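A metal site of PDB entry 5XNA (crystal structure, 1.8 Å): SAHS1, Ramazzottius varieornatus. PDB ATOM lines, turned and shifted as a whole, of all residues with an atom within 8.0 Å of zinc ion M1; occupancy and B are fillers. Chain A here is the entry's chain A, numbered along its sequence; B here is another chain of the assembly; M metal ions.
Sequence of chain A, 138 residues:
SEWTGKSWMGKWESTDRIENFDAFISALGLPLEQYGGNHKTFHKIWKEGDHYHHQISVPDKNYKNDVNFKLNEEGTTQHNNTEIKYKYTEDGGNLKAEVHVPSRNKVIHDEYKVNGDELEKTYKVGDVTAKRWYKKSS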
ATOM      1  N   ALA A  97     -10.098  28.176   8.806  1.00  0.00           N
ATOM      2  CA  ALA A  97     -11.419  27.777   9.256  1.00  0.00           C
ATOM      3  C   ALA A  97     -11.291  26.540  10.139  1.00  0.00           C
ATOM      4  O   ALA A  97     -10.602  25.576   9.762  1.00  0.00           O
ATOM      5  CB  ALA A  97     -12.355  27.493   8.081  1.00  0.00           C
ATOM      6  N   GLU A  98     -11.943  26.580  11.292  1.00  0.00           N
ATOM      7  CA  GLU A  98     -12.067  25.452  12.215  1.00  0.00           C
ATOM      8  C   GLU A  98     -13.451  24.842  12.030  1.00  0.00           C
ATOM      9  O   GLU A  98     -14.445  25.537  12.243  1.00  0.00           O
ATOM     10  CB  GLU A  98     -11.875  25.913  13.658  1.00  0.00           C
ATOM     11  CG  GLU A  98     -11.826  24.769  14.654  1.00  0.00           C
ATOM     12  CD  GLU A  98     -10.419  24.194  14.793  1.00  0.00           C
ATOM     13  OE1 GLU A  98      -9.470  24.798  14.247  1.00  0.00           O
ATOM     14  OE2 GLU A  98     -10.292  23.147  15.439  1.00  0.00           O
ATOM     15  N   VAL A  99     -13.522  23.581  11.612  1.00  0.00           N
ATOM     16  CA  VAL A  99     -14.799  22.980  11.223  1.00  0.00           C
ATOM     17  C   VAL A  99     -15.080  21.765  12.101  1.00  0.00           C
ATOM     18  O   VAL A  99     -14.252  20.856  12.191  1.00  0.00           O
ATOM     19  CB  VAL A  99     -14.796  22.586   9.737  1.00  0.00           C
ATOM     20  CG1 VAL A  99     -16.131  21.944   9.355  1.00  0.00           C
ATOM     21  CG2 VAL A  99     -14.502  23.803   8.871  1.00  0.00           C
ATOM     22  N   HIS A 100     -16.244  21.755  12.748  1.00  0.00           N
ATOM     23  CA  HIS A 100     -16.719  20.577  13.482  1.00  0.00           C
ATOM     24  C   HIS A 100     -17.754  19.843  12.648  1.00  0.00           C
ATOM     25  O   HIS A 100     -18.678  20.456  12.106  1.00  0.00           O
ATOM     26  CB  HIS A 100     -17.361  20.960  14.821  1.00  0.00           C
ATOM     27  CG  HIS A 100     -16.397  21.350  15.915  1.00  0.00           C
ATOM     28  ND1 HIS A 100     -15.788  22.587  15.969  1.00  0.00           N
ATOM     29  CD2 HIS A 100     -16.010  20.684  17.027  1.00  0.00           C
ATOM     30  CE1 HIS A 100     -15.047  22.659  17.061  1.00  0.00           C
ATOM     31  NE2 HIS A 100     -15.162  21.514  17.719  1.00  0.00           N
ATOM     32  N   VAL A 107     -12.978  16.823  13.293  1.00  0.00           N
ATOM     33  CA  VAL A 107     -12.550  18.225  13.294  1.00  0.00           C
ATOM     34  C   VAL A 107     -11.659  18.442  12.074  1.00  0.00           C
ATOM     35  O   VAL A 107     -10.655  17.739  11.901  1.00  0.00           O
ATOM     36  CB  VAL A 107     -11.814  18.600  14.582  1.00  0.00           C
ATOM     37  CG1 VAL A 107     -11.298  20.042  14.487  1.00  0.00           C
ATOM     38  CG2 VAL A 107     -12.706  18.412  15.808  1.00  0.00           C
ATOM     39  N   ILE A 108     -12.024  19.406  11.232  1.00  0.00           N
ATOM     40  CA  ILE A 108     -11.306  19.681   9.986  1.00  0.00           C
ATOM     41  C   ILE A 108     -10.677  21.062  10.087  1.00  0.00           C
ATOM     42  O   ILE A 108     -11.332  22.006  10.548  1.00  0.00           O
ATOM     43  CB  ILE A 108     -12.242  19.627   8.761  1.00  0.00           C
ATOM     44  CG1 ILE A 108     -12.885  18.257   8.606  1.00  0.00           C
ATOM     45  CG2 ILE A 108     -11.494  20.053   7.500  1.00  0.00           C
ATOM     46  CD1 ILE A 108     -14.031  18.243   7.627  1.00  0.00           C
ATOM     47  N   HIS A 109      -9.408  21.162   9.722  1.00  0.00           N
ATOM     48  CA  HIS A 109      -8.748  22.449   9.544  1.00  0.00           C
ATOM     49  C   HIS A 109      -8.698  22.799   8.064  1.00  0.00           C
ATOM     50  O   HIS A 109      -8.275  21.974   7.247  1.00  0.00           O
ATOM     51  CB  HIS A 109      -7.314  22.437  10.103  1.00  0.00           C
ATOM     52  CG  HIS A 109      -7.244  22.392  11.592  1.00  0.00           C
ATOM     53  ND1 HIS A 109      -6.060  22.213  12.269  1.00  0.00           N
ATOM     54  CD2 HIS A 109      -8.202  22.524  12.536  1.00  0.00           C
ATOM     55  CE1 HIS A 109      -6.293  22.214  13.576  1.00  0.00           C
ATOM     56  NE2 HIS A 109      -7.592  22.393  13.768  1.00  0.00           N
ATOM     57  N   ASP A 110      -9.128  24.013   7.721  1.00  0.00           N
ATOM     58  CA  ASP A 110      -8.903  24.603   6.410  1.00  0.00           C
ATOM     59  C   ASP A 110      -7.952  25.778   6.567  1.00  0.00           C
ATOM     60  O   ASP A 110      -8.048  26.523   7.553  1.00  0.00           O
ATOM     61  CB  ASP A 110     -10.195  25.118   5.784  1.00  0.00           C
ATOM     62  CG  ASP A 110     -11.188  24.042   5.509  1.00  0.00           C
ATOM     63  OD1 ASP A 110     -10.754  22.912   5.215  1.00  0.00           O
ATOM     64  OD2 ASP A 110     -12.398  24.329   5.589  1.00  0.00           O
ATOM     65  N   LYS A 124      -6.826  19.553   6.598  1.00  0.00           N
ATOM     66  CA  LYS A 124      -6.191  18.678   7.576  1.00  0.00           C
ATOM     67  C   LYS A 124      -7.220  18.100   8.526  1.00  0.00           C
ATOM     68  O   LYS A 124      -8.001  18.832   9.132  1.00  0.00           O
ATOM     69  CB  LYS A 124      -5.117  19.432   8.366  1.00  0.00           C
ATOM     70  CG  LYS A 124      -4.223  18.545   9.202  1.00  0.00           C
ATOM     71  CD  LYS A 124      -3.141  19.367   9.886  1.00  0.00           C
ATOM     72  CE  LYS A 124      -2.456  20.308   8.902  1.00  0.00           C
ATOM     73  NZ  LYS A 124      -1.417  21.169   9.560  1.00  0.00           N
ATOM     74  N   ALA B  97      -0.796  19.588  19.880  1.00  0.00           N
ATOM     75  CA  ALA B  97      -1.942  19.075  20.621  1.00  0.00           C
ATOM     76  C   ALA B  97      -3.192  19.840  20.191  1.00  0.00           C
ATOM     77  O   ALA B  97      -3.185  21.080  20.152  1.00  0.00           O
ATOM     78  CB  ALA B  97      -1.737  19.211  22.135  1.00  0.00           C
ATOM     79  N   GLU B  98      -4.221  19.106  19.809  1.00  0.00           N
ATOM     80  CA  GLU B  98      -5.532  19.641  19.460  1.00  0.00           C
ATOM     81  C   GLU B  98      -6.402  19.453  20.688  1.00  0.00           C
ATOM     82  O   GLU B  98      -6.653  18.322  21.093  1.00  0.00           O
ATOM     83  CB  GLU B  98      -6.101  18.875  18.272  1.00  0.00           C
ATOM     84  CG  GLU B  98      -7.474  19.332  17.811  1.00  0.00           C
ATOM     85  CD  GLU B  98      -7.396  20.564  16.950  1.00  0.00           C
ATOM     86  OE1 GLU B  98      -6.287  20.906  16.466  1.00  0.00           O
ATOM     87  OE2 GLU B  98      -8.450  21.199  16.765  1.00  0.00           O
ATOM     88  N   VAL B  99      -6.811  20.552  21.327  1.00  0.00           N
ATOM     89  CA  VAL B  99      -7.426  20.450  22.657  1.00  0.00           C
ATOM     90  C   VAL B  99      -8.794  21.109  22.577  1.00  0.00           C
ATOM     91  O   VAL B  99      -8.887  22.311  22.296  1.00  0.00           O
ATOM     92  CB  VAL B  99      -6.553  21.111  23.725  1.00  0.00           C
ATOM     93  CG1 VAL B  99      -7.221  21.036  25.081  1.00  0.00           C
ATOM     94  CG2 VAL B  99      -5.149  20.446  23.741  1.00  0.00           C
ATOM     95  N   HIS B 100      -9.839  20.338  22.816  1.00  0.00           N
ATOM     96  CA  HIS B 100     -11.197  20.850  22.741  1.00  0.00           C
ATOM     97  C   HIS B 100     -11.855  20.760  24.107  1.00  0.00           C
ATOM     98  O   HIS B 100     -11.734  19.748  24.814  1.00  0.00           O
ATOM     99  CB  HIS B 100     -12.011  20.112  21.688  1.00  0.00           C
ATOM    100  CG  HIS B 100     -11.593  20.406  20.276  1.00  0.00           C
ATOM    101  ND1 HIS B 100     -12.472  20.787  19.303  1.00  0.00           N
ATOM    102  CD2 HIS B 100     -10.363  20.390  19.696  1.00  0.00           C
ATOM    103  CE1 HIS B 100     -11.825  20.986  18.163  1.00  0.00           C
ATOM    104  NE2 HIS B 100     -10.543  20.742  18.378  1.00  0.00           N
ATOM    105  N   VAL B 107     -11.518  25.905  21.653  1.00  0.00           N
ATOM    106  CA  VAL B 107     -10.551  25.090  20.939  1.00  0.00           C
ATOM    107  C   VAL B 107      -9.183  25.700  21.158  1.00  0.00           C
ATOM    108  O   VAL B 107      -8.974  26.886  20.857  1.00  0.00           O
ATOM    109  CB  VAL B 107     -10.856  25.008  19.431  1.00  0.00           C
ATOM    110  CG1 VAL B 107      -9.738  24.208  18.734  1.00  0.00           C
ATOM    111  CG2 VAL B 107     -12.207  24.375  19.180  1.00  0.00           C
ATOM    112  N   ILE B 108      -8.242  24.901  21.636  1.00  0.00           N
ATOM    113  CA  ILE B 108      -6.878  25.352  21.876  1.00  0.00           C
ATOM    114  C   ILE B 108      -5.973  24.568  20.932  1.00  0.00           C
ATOM    115  O   ILE B 108      -6.107  23.343  20.834  1.00  0.00           O
ATOM    116  CB  ILE B 108      -6.462  25.120  23.344  1.00  0.00           C
ATOM    117  CG1 ILE B 108      -7.407  25.867  24.284  1.00  0.00           C
ATOM    118  CG2 ILE B 108      -4.975  25.477  23.535  1.00  0.00           C
ATOM    119  CD1 ILE B 108      -7.450  25.300  25.680  1.00  0.00           C
ATOM    120  N   HIS B 109      -5.089  25.268  20.243  1.00  0.00           N
ATOM    121  CA  HIS B 109      -4.040  24.653  19.423  1.00  0.00           C
ATOM    122  C   HIS B 109      -2.692  24.877  20.104  1.00  0.00           C
ATOM    123  O   HIS B 109      -2.232  26.013  20.191  1.00  0.00           O
ATOM    124  CB  HIS B 109      -4.000  25.247  18.011  1.00  0.00           C
ATOM    125  CG  HIS B 109      -5.208  24.931  17.187  1.00  0.00           C
ATOM    126  ND1 HIS B 109      -5.561  25.672  16.082  1.00  0.00           N
ATOM    127  CD2 HIS B 109      -6.120  23.928  17.271  1.00  0.00           C
ATOM    128  CE1 HIS B 109      -6.661  25.169  15.549  1.00  0.00           C
ATOM    129  NE2 HIS B 109      -7.019  24.112  16.248  1.00  0.00           N
HETATM  130 ZN    ZN M   1      -8.296  22.748  15.533  1.00  0.00          ZN
HETATM  131 ZN    ZN M   2     -14.545  21.036  19.554  1.00  0.00          ZN
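NE2 of His 109 of chain A binds zinc ion M1 (1.9 Å).
Zinc ion M1 is bound by OE2 of Glu 98 of chain B (2.0 Å).
Zinc ion M1 is bound by NE2 of His 109 of chain B, 2.0 Å away.
OE2 of Glu 98 of chain A binds zinc ion M1 (2.0 Å).
Slightly farther from zinc ion M1 lies the side-chain carboxylate (OE1) of Glu 98 of chain A (2.7 Å).
CG1 of Val 107 of chain B touches zinc ion M1, 3.8 Å away.
Five residues have an atom within 4 Å of zinc ion M1: Glu 98 of chain A, His 109 of chain A, Glu 98 of chain B, Val 107 of chain B and His 109 of chain B.
The backbone carbonyl oxygen of Lys 124 is in hydrogen-bond range of the backbone NH of His 109 of chain A, at 2.8 Å.
A ring nitrogen (NE2) of His 100 of chain B lies close to the side-chain carboxylate (OE2) of Glu 98 of chain B (2.7 Å).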
